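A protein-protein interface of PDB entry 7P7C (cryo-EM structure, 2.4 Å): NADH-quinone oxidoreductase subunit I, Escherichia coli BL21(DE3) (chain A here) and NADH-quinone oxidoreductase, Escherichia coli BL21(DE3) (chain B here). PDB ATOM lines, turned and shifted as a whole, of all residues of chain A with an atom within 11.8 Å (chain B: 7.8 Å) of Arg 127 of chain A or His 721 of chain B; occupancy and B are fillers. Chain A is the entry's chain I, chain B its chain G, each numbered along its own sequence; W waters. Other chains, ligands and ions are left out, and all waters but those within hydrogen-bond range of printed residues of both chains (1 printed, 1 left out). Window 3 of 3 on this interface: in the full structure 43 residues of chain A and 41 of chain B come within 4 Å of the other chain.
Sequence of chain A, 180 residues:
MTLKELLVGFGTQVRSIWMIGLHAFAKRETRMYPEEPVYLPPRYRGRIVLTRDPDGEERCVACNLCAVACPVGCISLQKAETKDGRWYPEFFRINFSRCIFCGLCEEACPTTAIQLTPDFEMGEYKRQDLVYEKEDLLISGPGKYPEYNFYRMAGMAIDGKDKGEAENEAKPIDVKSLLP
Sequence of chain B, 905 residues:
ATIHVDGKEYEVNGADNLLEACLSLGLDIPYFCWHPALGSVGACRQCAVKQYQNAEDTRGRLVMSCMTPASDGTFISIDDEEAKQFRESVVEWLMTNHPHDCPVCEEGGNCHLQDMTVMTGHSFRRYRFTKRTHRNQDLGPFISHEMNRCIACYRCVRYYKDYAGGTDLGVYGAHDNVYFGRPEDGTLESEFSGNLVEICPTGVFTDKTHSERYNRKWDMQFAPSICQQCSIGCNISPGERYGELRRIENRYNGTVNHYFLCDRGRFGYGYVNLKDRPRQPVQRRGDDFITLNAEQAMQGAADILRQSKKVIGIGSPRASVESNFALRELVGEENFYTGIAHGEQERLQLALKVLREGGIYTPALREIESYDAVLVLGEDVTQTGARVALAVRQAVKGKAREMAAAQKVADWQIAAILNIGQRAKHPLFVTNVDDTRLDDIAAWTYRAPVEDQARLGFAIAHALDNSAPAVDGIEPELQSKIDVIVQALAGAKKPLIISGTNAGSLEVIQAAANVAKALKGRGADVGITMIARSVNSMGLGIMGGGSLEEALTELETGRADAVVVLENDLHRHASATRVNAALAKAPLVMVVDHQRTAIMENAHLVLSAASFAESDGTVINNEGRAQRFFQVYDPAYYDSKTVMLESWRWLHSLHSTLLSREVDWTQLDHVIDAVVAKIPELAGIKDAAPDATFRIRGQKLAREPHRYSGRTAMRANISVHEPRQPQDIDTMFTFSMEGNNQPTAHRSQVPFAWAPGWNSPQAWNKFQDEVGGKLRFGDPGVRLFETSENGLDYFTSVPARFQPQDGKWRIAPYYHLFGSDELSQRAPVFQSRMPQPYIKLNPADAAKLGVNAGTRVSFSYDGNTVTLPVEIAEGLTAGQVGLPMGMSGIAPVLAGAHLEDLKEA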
ATOM      1  N   VAL A  72       3.752 -39.306  -7.117  1.00  0.00           N
ATOM      2  CA  VAL A  72       3.543 -38.009  -6.493  1.00  0.00           C
ATOM      3  C   VAL A  72       2.905 -37.020  -7.460  1.00  0.00           C
ATOM      4  O   VAL A  72       2.273 -36.051  -7.019  1.00  0.00           O
ATOM      5  CB  VAL A  72       4.889 -37.490  -5.950  1.00  0.00           C
ATOM      6  CG1 VAL A  72       4.697 -36.349  -4.979  1.00  0.00           C
ATOM      7  CG2 VAL A  72       5.638 -38.618  -5.270  1.00  0.00           C
ATOM      8  N   GLY A  73       3.004 -37.266  -8.761  1.00  0.00           N
ATOM      9  CA  GLY A  73       2.511 -36.335  -9.755  1.00  0.00           C
ATOM     10  C   GLY A  73       3.303 -35.051  -9.834  1.00  0.00           C
ATOM     11  O   GLY A  73       2.716 -33.974  -9.985  1.00  0.00           O
ATOM     12  N   CYS A  74       4.627 -35.133  -9.739  1.00  0.00           N
ATOM     13  CA  CYS A  74       5.478 -33.953  -9.738  1.00  0.00           C
ATOM     14  C   CYS A  74       6.220 -33.765 -11.058  1.00  0.00           C
ATOM     15  O   CYS A  74       7.254 -33.104 -11.097  1.00  0.00           O
ATOM     16  CB  CYS A  74       6.462 -34.002  -8.571  1.00  0.00           C
ATOM     17  SG  CYS A  74       7.609 -35.382  -8.584  1.00  0.00           S
ATOM     18  N   ARG A  93       8.880 -29.756 -16.478  1.00  0.00           N
ATOM     19  CA  ARG A  93       9.199 -29.286 -15.144  1.00  0.00           C
ATOM     20  C   ARG A  93       8.968 -30.393 -14.129  1.00  0.00           C
ATOM     21  O   ARG A  93       8.057 -31.217 -14.273  1.00  0.00           O
ATOM     22  CB  ARG A  93       8.407 -28.013 -14.787  1.00  0.00           C
ATOM     23  CG  ARG A  93       7.043 -28.199 -14.170  1.00  0.00           C
ATOM     24  CD  ARG A  93       6.487 -26.854 -13.747  1.00  0.00           C
ATOM     25  NE  ARG A  93       6.302 -25.972 -14.892  1.00  0.00           N
ATOM     26  CZ  ARG A  93       5.181 -25.877 -15.591  1.00  0.00           C
ATOM     27  NH1 ARG A  93       4.106 -26.574 -15.268  1.00  0.00           N
ATOM     28  NH2 ARG A  93       5.139 -25.063 -16.641  1.00  0.00           N
ATOM     29  N   ILE A  94       9.846 -30.430 -13.132  1.00  0.00           N
ATOM     30  CA  ILE A  94       9.792 -31.396 -12.048  1.00  0.00           C
ATOM     31  C   ILE A  94       9.833 -30.628 -10.737  1.00  0.00           C
ATOM     32  O   ILE A  94      10.781 -29.878 -10.482  1.00  0.00           O
ATOM     33  CB  ILE A  94      10.943 -32.412 -12.115  1.00  0.00           C
ATOM     34  CG1 ILE A  94      10.869 -33.210 -13.415  1.00  0.00           C
ATOM     35  CG2 ILE A  94      10.908 -33.340 -10.911  1.00  0.00           C
ATOM     36  CD1 ILE A  94      12.108 -33.976 -13.716  1.00  0.00           C
ATOM     37  N   ASN A  95       8.809 -30.811  -9.913  1.00  0.00           N
ATOM     38  CA  ASN A  95       8.777 -30.238  -8.573  1.00  0.00           C
ATOM     39  C   ASN A  95       9.601 -31.146  -7.671  1.00  0.00           C
ATOM     40  O   ASN A  95       9.133 -32.201  -7.238  1.00  0.00           O
ATOM     41  CB  ASN A  95       7.338 -30.106  -8.088  1.00  0.00           C
ATOM     42  CG  ASN A  95       7.215 -29.312  -6.804  1.00  0.00           C
ATOM     43  OD1 ASN A  95       8.206 -28.875  -6.224  1.00  0.00           O
ATOM     44  ND2 ASN A  95       5.985 -29.123  -6.352  1.00  0.00           N
ATOM     45  N   PHE A  96      10.839 -30.746  -7.394  1.00  0.00           N
ATOM     46  CA  PHE A  96      11.720 -31.564  -6.572  1.00  0.00           C
ATOM     47  C   PHE A  96      11.432 -31.440  -5.085  1.00  0.00           C
ATOM     48  O   PHE A  96      11.961 -32.236  -4.305  1.00  0.00           O
ATOM     49  CB  PHE A  96      13.180 -31.213  -6.847  1.00  0.00           C
ATOM     50  CG  PHE A  96      13.751 -31.926  -8.029  1.00  0.00           C
ATOM     51  CD1 PHE A  96      13.824 -33.306  -8.053  1.00  0.00           C
ATOM     52  CD2 PHE A  96      14.205 -31.218  -9.126  1.00  0.00           C
ATOM     53  CE1 PHE A  96      14.347 -33.963  -9.143  1.00  0.00           C
ATOM     54  CE2 PHE A  96      14.727 -31.870 -10.219  1.00  0.00           C
ATOM     55  CZ  PHE A  96      14.799 -33.241 -10.227  1.00  0.00           C
ATOM     56  N   SER A  97      10.616 -30.470  -4.671  1.00  0.00           N
ATOM     57  CA  SER A  97      10.148 -30.451  -3.294  1.00  0.00           C
ATOM     58  C   SER A  97       9.147 -31.564  -3.025  1.00  0.00           C
ATOM     59  O   SER A  97       8.957 -31.945  -1.868  1.00  0.00           O
ATOM     60  CB  SER A  97       9.531 -29.091  -2.960  1.00  0.00           C
ATOM     61  OG  SER A  97       8.270 -28.923  -3.578  1.00  0.00           O
ATOM     62  N   ARG A  98       8.507 -32.090  -4.068  1.00  0.00           N
ATOM     63  CA  ARG A  98       7.593 -33.216  -3.950  1.00  0.00           C
ATOM     64  C   ARG A  98       8.238 -34.550  -4.285  1.00  0.00           C
ATOM     65  O   ARG A  98       7.782 -35.581  -3.786  1.00  0.00           O
ATOM     66  CB  ARG A  98       6.383 -33.016  -4.868  1.00  0.00           C
ATOM     67  CG  ARG A  98       5.351 -32.046  -4.348  1.00  0.00           C
ATOM     68  CD  ARG A  98       4.334 -32.750  -3.482  1.00  0.00           C
ATOM     69  NE  ARG A  98       3.210 -31.887  -3.146  1.00  0.00           N
ATOM     70  CZ  ARG A  98       2.255 -32.206  -2.285  1.00  0.00           C
ATOM     71  NH1 ARG A  98       2.263 -33.362  -1.641  1.00  0.00           N
ATOM     72  NH2 ARG A  98       1.269 -31.344  -2.061  1.00  0.00           N
ATOM     73  N   CYS A  99       9.281 -34.544  -5.114  1.00  0.00           N
ATOM     74  CA  CYS A  99       9.832 -35.775  -5.670  1.00  0.00           C
ATOM     75  C   CYS A  99      10.459 -36.640  -4.585  1.00  0.00           C
ATOM     76  O   CYS A  99      11.226 -36.154  -3.749  1.00  0.00           O
ATOM     77  CB  CYS A  99      10.869 -35.449  -6.740  1.00  0.00           C
ATOM     78  SG  CYS A  99      11.856 -36.856  -7.267  1.00  0.00           S
ATOM     79  N   MET A 122      21.263 -31.245  -3.515  1.00  0.00           N
ATOM     80  CA  MET A 122      20.198 -30.457  -4.121  1.00  0.00           C
ATOM     81  C   MET A 122      19.515 -29.529  -3.122  1.00  0.00           C
ATOM     82  O   MET A 122      18.388 -29.092  -3.370  1.00  0.00           O
ATOM     83  CB  MET A 122      19.159 -31.368  -4.771  1.00  0.00           C
ATOM     84  CG  MET A 122      19.686 -32.307  -5.827  1.00  0.00           C
ATOM     85  SD  MET A 122      18.384 -33.426  -6.362  1.00  0.00           S
ATOM     86  CE  MET A 122      17.207 -32.271  -7.051  1.00  0.00           C
ATOM     87  N   GLY A 123      20.171 -29.220  -2.005  1.00  0.00           N
ATOM     88  CA  GLY A 123      19.570 -28.351  -1.011  1.00  0.00           C
ATOM     89  C   GLY A 123      19.365 -26.940  -1.527  1.00  0.00           C
ATOM     90  O   GLY A 123      20.126 -26.432  -2.348  1.00  0.00           O
ATOM     91  N   GLU A 124      18.310 -26.298  -1.031  1.00  0.00           N
ATOM     92  CA  GLU A 124      17.837 -25.043  -1.593  1.00  0.00           C
ATOM     93  C   GLU A 124      17.377 -24.118  -0.477  1.00  0.00           C
ATOM     94  O   GLU A 124      17.010 -24.561   0.612  1.00  0.00           O
ATOM     95  CB  GLU A 124      16.697 -25.292  -2.587  1.00  0.00           C
ATOM     96  CG  GLU A 124      16.507 -24.214  -3.626  1.00  0.00           C
ATOM     97  CD  GLU A 124      17.747 -23.975  -4.455  1.00  0.00           C
ATOM     98  OE1 GLU A 124      18.011 -24.777  -5.372  1.00  0.00           O
ATOM     99  OE2 GLU A 124      18.454 -22.981  -4.190  1.00  0.00           O
ATOM    100  N   TYR A 125      17.402 -22.815  -0.764  1.00  0.00           N
ATOM    101  CA  TYR A 125      16.931 -21.801   0.171  1.00  0.00           C
ATOM    102  C   TYR A 125      15.436 -21.535   0.038  1.00  0.00           C
ATOM    103  O   TYR A 125      14.738 -21.420   1.048  1.00  0.00           O
ATOM    104  CB  TYR A 125      17.706 -20.497  -0.031  1.00  0.00           C
ATOM    105  CG  TYR A 125      19.154 -20.580   0.376  1.00  0.00           C
ATOM    106  CD1 TYR A 125      19.511 -20.744   1.706  1.00  0.00           C
ATOM    107  CD2 TYR A 125      20.167 -20.497  -0.568  1.00  0.00           C
ATOM    108  CE1 TYR A 125      20.832 -20.821   2.084  1.00  0.00           C
ATOM    109  CE2 TYR A 125      21.491 -20.572  -0.200  1.00  0.00           C
ATOM    110  CZ  TYR A 125      21.818 -20.736   1.128  1.00  0.00           C
ATOM    111  OH  TYR A 125      23.137 -20.813   1.504  1.00  0.00           O
ATOM    112  N   LYS A 126      14.932 -21.432  -1.187  1.00  0.00           N
ATOM    113  CA  LYS A 126      13.523 -21.181  -1.444  1.00  0.00           C
ATOM    114  C   LYS A 126      12.897 -22.396  -2.114  1.00  0.00           C
ATOM    115  O   LYS A 126      13.496 -23.001  -3.007  1.00  0.00           O
ATOM    116  CB  LYS A 126      13.338 -19.945  -2.326  1.00  0.00           C
ATOM    117  CG  LYS A 126      14.059 -18.710  -1.825  1.00  0.00           C
ATOM    118  CD  LYS A 126      13.158 -17.871  -0.938  1.00  0.00           C
ATOM    119  CE  LYS A 126      13.946 -17.208   0.177  1.00  0.00           C
ATOM    120  NZ  LYS A 126      14.427 -15.854  -0.211  1.00  0.00           N
ATOM    121  N   ARG A 127      11.686 -22.746  -1.677  1.00  0.00           N
ATOM    122  CA  ARG A 127      11.019 -23.939  -2.187  1.00  0.00           C
ATOM    123  C   ARG A 127      10.594 -23.784  -3.643  1.00  0.00           C
ATOM    124  O   ARG A 127      10.513 -24.780  -4.369  1.00  0.00           O
ATOM    125  CB  ARG A 127       9.814 -24.269  -1.312  1.00  0.00           C
ATOM    126  CG  ARG A 127       9.282 -25.672  -1.488  1.00  0.00           C
ATOM    127  CD  ARG A 127       8.104 -25.905  -0.583  1.00  0.00           C
ATOM    128  NE  ARG A 127       6.979 -26.512  -1.280  1.00  0.00           N
ATOM    129  CZ  ARG A 127       5.715 -26.384  -0.903  1.00  0.00           C
ATOM    130  NH1 ARG A 127       5.381 -25.679   0.162  1.00  0.00           N
ATOM    131  NH2 ARG A 127       4.764 -26.980  -1.613  1.00  0.00           N
ATOM    132  N   GLN A 128      10.317 -22.552  -4.083  1.00  0.00           N
ATOM    133  CA  GLN A 128       9.997 -22.309  -5.487  1.00  0.00           C
ATOM    134  C   GLN A 128      11.173 -22.638  -6.397  1.00  0.00           C
ATOM    135  O   GLN A 128      10.976 -23.063  -7.540  1.00  0.00           O
ATOM    136  CB  GLN A 128       9.563 -20.854  -5.673  1.00  0.00           C
ATOM    137  CG  GLN A 128       9.101 -20.496  -7.072  1.00  0.00           C
ATOM    138  CD  GLN A 128       7.887 -21.286  -7.500  1.00  0.00           C
ATOM    139  OE1 GLN A 128       6.920 -21.408  -6.754  1.00  0.00           O
ATOM    140  NE2 GLN A 128       7.932 -21.829  -8.708  1.00  0.00           N
ATOM    141  N   ASP A 129      12.401 -22.483  -5.899  1.00  0.00           N
ATOM    142  CA  ASP A 129      13.593 -22.806  -6.672  1.00  0.00           C
ATOM    143  C   ASP A 129      13.843 -24.305  -6.789  1.00  0.00           C
ATOM    144  O   ASP A 129      14.773 -24.704  -7.494  1.00  0.00           O
ATOM    145  CB  ASP A 129      14.806 -22.118  -6.055  1.00  0.00           C
ATOM    146  CG  ASP A 129      14.815 -20.628  -6.305  1.00  0.00           C
ATOM    147  OD1 ASP A 129      14.389 -20.208  -7.401  1.00  0.00           O
ATOM    148  OD2 ASP A 129      15.243 -19.873  -5.407  1.00  0.00           O
ATOM    149  N   LEU A 130      13.052 -25.138  -6.117  1.00  0.00           N
ATOM    150  CA  LEU A 130      13.096 -26.580  -6.318  1.00  0.00           C
ATOM    151  C   LEU A 130      12.240 -27.034  -7.492  1.00  0.00           C
ATOM    152  O   LEU A 130      12.159 -28.237  -7.750  1.00  0.00           O
ATOM    153  CB  LEU A 130      12.657 -27.304  -5.045  1.00  0.00           C
ATOM    154  CG  LEU A 130      13.679 -27.307  -3.909  1.00  0.00           C
ATOM    155  CD1 LEU A 130      13.097 -27.940  -2.662  1.00  0.00           C
ATOM    156  CD2 LEU A 130      14.937 -28.033  -4.343  1.00  0.00           C
ATOM    157  N   VAL A 131      11.590 -26.109  -8.195  1.00  0.00           N
ATOM    158  CA  VAL A 131      10.890 -26.417  -9.436  1.00  0.00           C
ATOM    159  C   VAL A 131      11.914 -26.288 -10.559  1.00  0.00           C
ATOM    160  O   VAL A 131      12.319 -25.186 -10.926  1.00  0.00           O
ATOM    161  CB  VAL A 131       9.687 -25.497  -9.653  1.00  0.00           C
ATOM    162  CG1 VAL A 131       8.945 -25.890 -10.915  1.00  0.00           C
ATOM    163  CG2 VAL A 131       8.760 -25.547  -8.451  1.00  0.00           C
ATOM    164  N   TYR A 132      12.337 -27.424 -11.107  1.00  0.00           N
ATOM    165  CA  TYR A 132      13.365 -27.456 -12.138  1.00  0.00           C
ATOM    166  C   TYR A 132      12.700 -27.517 -13.506  1.00  0.00           C
ATOM    167  O   TYR A 132      12.029 -28.500 -13.825  1.00  0.00           O
ATOM    168  CB  TYR A 132      14.285 -28.661 -11.953  1.00  0.00           C
ATOM    169  CG  TYR A 132      15.416 -28.475 -10.970  1.00  0.00           C
ATOM    170  CD1 TYR A 132      15.193 -27.932  -9.710  1.00  0.00           C
ATOM    171  CD2 TYR A 132      16.706 -28.865 -11.293  1.00  0.00           C
ATOM    172  CE1 TYR A 132      16.221 -27.775  -8.813  1.00  0.00           C
ATOM    173  CE2 TYR A 132      17.741 -28.710 -10.402  1.00  0.00           C
ATOM    174  CZ  TYR A 132      17.494 -28.163  -9.163  1.00  0.00           C
ATOM    175  OH  TYR A 132      18.524 -28.007  -8.271  1.00  0.00           O
ATOM    176  N   GLU A 133      12.904 -26.486 -14.317  1.00  0.00           N
ATOM    177  CA  GLU A 133      12.359 -26.461 -15.667  1.00  0.00           C
ATOM    178  C   GLU A 133      13.305 -27.205 -16.606  1.00  0.00           C
ATOM    179  O   GLU A 133      14.297 -27.800 -16.182  1.00  0.00           O
ATOM    180  CB  GLU A 133      12.113 -25.025 -16.117  1.00  0.00           C
ATOM    181  CG  GLU A 133      11.208 -24.232 -15.195  1.00  0.00           C
ATOM    182  CD  GLU A 133       9.738 -24.485 -15.455  1.00  0.00           C
ATOM    183  OE1 GLU A 133       9.386 -24.826 -16.602  1.00  0.00           O
ATOM    184  OE2 GLU A 133       8.932 -24.340 -14.514  1.00  0.00           O
ATOM    185  N   ASP A 136      17.066 -26.572 -16.605  1.00  0.00           N
ATOM    186  CA  ASP A 136      17.796 -27.102 -15.462  1.00  0.00           C
ATOM    187  C   ASP A 136      17.958 -28.615 -15.502  1.00  0.00           C
ATOM    188  O   ASP A 136      18.666 -29.166 -14.656  1.00  0.00           O
ATOM    189  CB  ASP A 136      17.091 -26.710 -14.163  1.00  0.00           C
ATOM    190  CG  ASP A 136      16.719 -25.244 -14.124  1.00  0.00           C
ATOM    191  OD1 ASP A 136      17.636 -24.399 -14.066  1.00  0.00           O
ATOM    192  OD2 ASP A 136      15.509 -24.938 -14.145  1.00  0.00           O
ATOM    193  N   ARG B 711      -0.452 -33.374 -10.800  1.00  0.00           N
ATOM    194  CA  ARG B 711      -1.249 -32.521  -9.925  1.00  0.00           C
ATOM    195  C   ARG B 711      -0.410 -31.662  -8.986  1.00  0.00           C
ATOM    196  O   ARG B 711      -0.909 -30.648  -8.493  1.00  0.00           O
ATOM    197  CB  ARG B 711      -2.225 -33.367  -9.111  1.00  0.00           C
ATOM    198  CG  ARG B 711      -1.571 -34.425  -8.250  1.00  0.00           C
ATOM    199  CD  ARG B 711      -2.579 -35.495  -7.887  1.00  0.00           C
ATOM    200  NE  ARG B 711      -3.704 -34.920  -7.163  1.00  0.00           N
ATOM    201  CZ  ARG B 711      -3.693 -34.645  -5.867  1.00  0.00           C
ATOM    202  NH1 ARG B 711      -2.649 -34.936  -5.109  1.00  0.00           N
ATOM    203  NH2 ARG B 711      -4.755 -34.063  -5.318  1.00  0.00           N
ATOM    204  N   THR B 712       0.841 -32.032  -8.722  1.00  0.00           N
ATOM    205  CA  THR B 712       1.728 -31.195  -7.927  1.00  0.00           C
ATOM    206  C   THR B 712       2.776 -30.487  -8.772  1.00  0.00           C
ATOM    207  O   THR B 712       3.747 -29.960  -8.222  1.00  0.00           O
ATOM    208  CB  THR B 712       2.411 -32.015  -6.827  1.00  0.00           C
ATOM    209  OG1 THR B 712       3.236 -33.026  -7.413  1.00  0.00           O
ATOM    210  CG2 THR B 712       1.379 -32.664  -5.935  1.00  0.00           C
ATOM    211  N   ARG B 715       0.914 -26.445 -11.999  1.00  0.00           N
ATOM    212  CA  ARG B 715       0.924 -25.036 -11.636  1.00  0.00           C
ATOM    213  C   ARG B 715       2.193 -24.633 -10.900  1.00  0.00           C
ATOM    214  O   ARG B 715       2.262 -23.520 -10.374  1.00  0.00           O
ATOM    215  CB  ARG B 715      -0.292 -24.699 -10.774  1.00  0.00           C
ATOM    216  CG  ARG B 715      -1.561 -24.436 -11.540  1.00  0.00           C
ATOM    217  CD  ARG B 715      -2.602 -23.799 -10.641  1.00  0.00           C
ATOM    218  NE  ARG B 715      -2.490 -22.345 -10.614  1.00  0.00           N
ATOM    219  CZ  ARG B 715      -2.132 -21.636  -9.552  1.00  0.00           C
ATOM    220  NH1 ARG B 715      -1.829 -22.215  -8.403  1.00  0.00           N
ATOM    221  NH2 ARG B 715      -2.074 -20.312  -9.649  1.00  0.00           N
ATOM    222  N   ALA B 716       3.197 -25.513 -10.848  1.00  0.00           N
ATOM    223  CA  ALA B 716       4.380 -25.265 -10.033  1.00  0.00           C
ATOM    224  C   ALA B 716       5.250 -24.137 -10.572  1.00  0.00           C
ATOM    225  O   ALA B 716       6.038 -23.570  -9.809  1.00  0.00           O
ATOM    226  CB  ALA B 716       5.206 -26.542  -9.903  1.00  0.00           C
ATOM    227  N   ILE B 718       3.934 -21.318 -11.621  1.00  0.00           N
ATOM    228  CA  ILE B 718       3.297 -20.152 -11.017  1.00  0.00           C
ATOM    229  C   ILE B 718       3.644 -20.075  -9.536  1.00  0.00           C
ATOM    230  O   ILE B 718       4.246 -19.102  -9.067  1.00  0.00           O
ATOM    231  CB  ILE B 718       1.774 -20.197 -11.237  1.00  0.00           C
ATOM    232  CG1 ILE B 718       1.449 -20.186 -12.732  1.00  0.00           C
ATOM    233  CG2 ILE B 718       1.093 -19.046 -10.522  1.00  0.00           C
ATOM    234  CD1 ILE B 718       2.081 -19.043 -13.486  1.00  0.00           C
ATOM    235  N   SER B 719       3.277 -21.107  -8.781  1.00  0.00           N
ATOM    236  CA  SER B 719       3.652 -21.207  -7.380  1.00  0.00           C
ATOM    237  C   SER B 719       3.798 -22.675  -7.015  1.00  0.00           C
ATOM    238  O   SER B 719       3.034 -23.518  -7.489  1.00  0.00           O
ATOM    239  CB  SER B 719       2.623 -20.532  -6.467  1.00  0.00           C
ATOM    240  OG  SER B 719       1.424 -21.278  -6.410  1.00  0.00           O
ATOM    241  N   VAL B 720       4.785 -22.971  -6.168  1.00  0.00           N
ATOM    242  CA  VAL B 720       5.013 -24.342  -5.731  1.00  0.00           C
ATOM    243  C   VAL B 720       3.916 -24.815  -4.783  1.00  0.00           C
ATOM    244  O   VAL B 720       3.737 -26.022  -4.597  1.00  0.00           O
ATOM    245  CB  VAL B 720       6.417 -24.455  -5.100  1.00  0.00           C
ATOM    246  CG1 VAL B 720       6.433 -23.898  -3.686  1.00  0.00           C
ATOM    247  CG2 VAL B 720       6.923 -25.892  -5.135  1.00  0.00           C
ATOM    248  N   HIS B 721       3.159 -23.893  -4.194  1.00  0.00           N
ATOM    249  CA  HIS B 721       2.056 -24.253  -3.316  1.00  0.00           C
ATOM    250  C   HIS B 721       0.837 -24.595  -4.162  1.00  0.00           C
ATOM    251  O   HIS B 721       0.367 -23.763  -4.945  1.00  0.00           O
ATOM    252  CB  HIS B 721       1.750 -23.107  -2.356  1.00  0.00           C
ATOM    253  CG  HIS B 721       2.936 -22.658  -1.560  1.00  0.00           C
ATOM    254  ND1 HIS B 721       3.220 -23.151  -0.305  1.00  0.00           N
ATOM    255  CD2 HIS B 721       3.918 -21.772  -1.846  1.00  0.00           C
ATOM    256  CE1 HIS B 721       4.320 -22.581   0.150  1.00  0.00           C
ATOM    257  NE2 HIS B 721       4.765 -21.742  -0.767  1.00  0.00           N
ATOM    258  N   GLU B 722       0.341 -25.816  -4.011  1.00  0.00           N
ATOM    259  CA  GLU B 722      -0.805 -26.266  -4.789  1.00  0.00           C
ATOM    260  C   GLU B 722      -2.054 -25.494  -4.381  1.00  0.00           C
ATOM    261  O   GLU B 722      -2.305 -25.318  -3.184  1.00  0.00           O
ATOM    262  CB  GLU B 722      -1.035 -27.764  -4.595  1.00  0.00           C
ATOM    263  CG  GLU B 722       0.013 -28.644  -5.239  1.00  0.00           C
ATOM    264  CD  GLU B 722       1.192 -28.901  -4.328  1.00  0.00           C
ATOM    265  OE1 GLU B 722       1.055 -28.698  -3.105  1.00  0.00           O
ATOM    266  OE2 GLU B 722       2.261 -29.298  -4.836  1.00  0.00           O
ATOM    267  N   PRO B 723      -2.853 -25.023  -5.330  1.00  0.00           N
ATOM    268  CA  PRO B 723      -4.105 -24.354  -4.982  1.00  0.00           C
ATOM    269  C   PRO B 723      -5.151 -25.367  -4.543  1.00  0.00           C
ATOM    270  O   PRO B 723      -4.986 -26.580  -4.677  1.00  0.00           O
ATOM    271  CB  PRO B 723      -4.507 -23.676  -6.290  1.00  0.00           C
ATOM    272  CG  PRO B 723      -3.991 -24.594  -7.326  1.00  0.00           C
ATOM    273  CD  PRO B 723      -2.685 -25.136  -6.788  1.00  0.00           C
ATOM    274  N   ARG B 724      -6.242 -24.839  -4.001  1.00  0.00           N
ATOM    275  CA  ARG B 724      -7.368 -25.681  -3.639  1.00  0.00           C
ATOM    276  C   ARG B 724      -8.020 -26.255  -4.889  1.00  0.00           C
ATOM    277  O   ARG B 724      -7.949 -25.677  -5.977  1.00  0.00           O
ATOM    278  CB  ARG B 724      -8.391 -24.884  -2.832  1.00  0.00           C
ATOM    279  CG  ARG B 724      -8.449 -23.414  -3.205  1.00  0.00           C
ATOM    280  CD  ARG B 724      -9.774 -22.788  -2.798  1.00  0.00           C
ATOM    281  NE  ARG B 724     -10.115 -21.640  -3.629  1.00  0.00           N
ATOM    282  CZ  ARG B 724     -10.616 -21.719  -4.855  1.00  0.00           C
ATOM    283  NH1 ARG B 724     -10.871 -22.885  -5.427  1.00  0.00           N
ATOM    284  NH2 ARG B 724     -10.878 -20.597  -5.522  1.00  0.00           N
HETATM  285  O   HOH W   1       2.803 -28.309  -1.204  1.00  0.00           O
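No residue of chain A comes within 4 Å of Arg 715 of chain B. Of chain A, only Gln 128 (3.3 Å) comes within 4 Å of Ser 719 of chain B. No residue of chain A comes within 4 Å of Pro 723 of chain B. Of the printed residues of chain B, Gly 73 of chain A touches Arg 711 (3.3 Å) and Thr 712 (2.8 Å). Of the printed residues of chain B, Cys 74 of chain A touches Thr 712. The nearest residue of chain B that does not touch Arg 127 of chain A is Glu 722 of chain B (4.4 Å). The nearest residue of chain A that does not touch His 721 of chain B is Gln 128 of chain A (5.2 Å). The nearest printed residue of chain B that does not touch Ser 97 of chain A is Glu 722 of chain B (6.2 Å).
The side-chain hydroxyl (OG) of Ser 719 of chain B is in hydrogen-bond range of the backbone carbonyl oxygen (O) of His 721 of chain B (3.1 Å). OG of Ser 97 of chain A sits at hydrogen-bond distance from OD1 of Asn 95 of chain A, 2.6 Å away.
Water W1 lies within hydrogen-bond range of NH2 of Arg 127 of chain A and OE1 of Glu 722 of chain B.
Ser 97 of chain A touches Val 720 of chain B (OG to CG2, 3.7 Å). NE of Arg 98 of chain A touches CG2 of Thr 712 of chain B, at 3.4 Å. Ser 719 of chain B touches Gln 128 of chain A. Val 131 of chain A touches Ala 716 of chain B (CG2 to O, 3.6 Å).
Hydrophobic or aromatic side chains of chain A that line the printed part of chain B: Val 131. Along chain A the printed residues that touch a printed residue of chain B span positions 72 to 131. Among the printed residues, 16 pairs touch across the chains. Among the printed residues, Asp or Glu carboxylates within 4 Å of a Lys or Arg side-chain nitrogen of the other chain: Arg 98 of chain A with Glu 722 of chain B (2.9 Å).
The backbone carbonyl oxygen (O) of Gly 73 of chain A lies within hydrogen-bond range of the backbone NH (N) of Arg 711 of chain B (3.3 Å). The backbone carbonyl oxygen (O) of Val 72 of chain A sits at hydrogen-bond distance from the side-chain hydroxyl (OG1) of Thr 712 of chain B, at 3.2 Å. OG1 of Thr 712 of chain B is in hydrogen-bond range of O of Gly 73 of chain A, 2.8 Å away. ND2 of Asn 95 of chain A lies within hydrogen-bond range of O of Thr 712 of chain B (3.0 Å). The guanidinium group (NH2) of Arg 127 of chain A sits at hydrogen-bond distance from the backbone carbonyl oxygen (O) of Val 720 of chain B (3.3 Å). The backbone NH (N) of Val 720 of chain B is in hydrogen-bond range of the side-chain amide oxygen (OE1) of Gln 128 of chain A (2.7 Å). The guanidinium group (NH1) of Arg 127 of chain A lies close to a ring nitrogen (ND1) of His 721 of chain B (3.4 Å).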
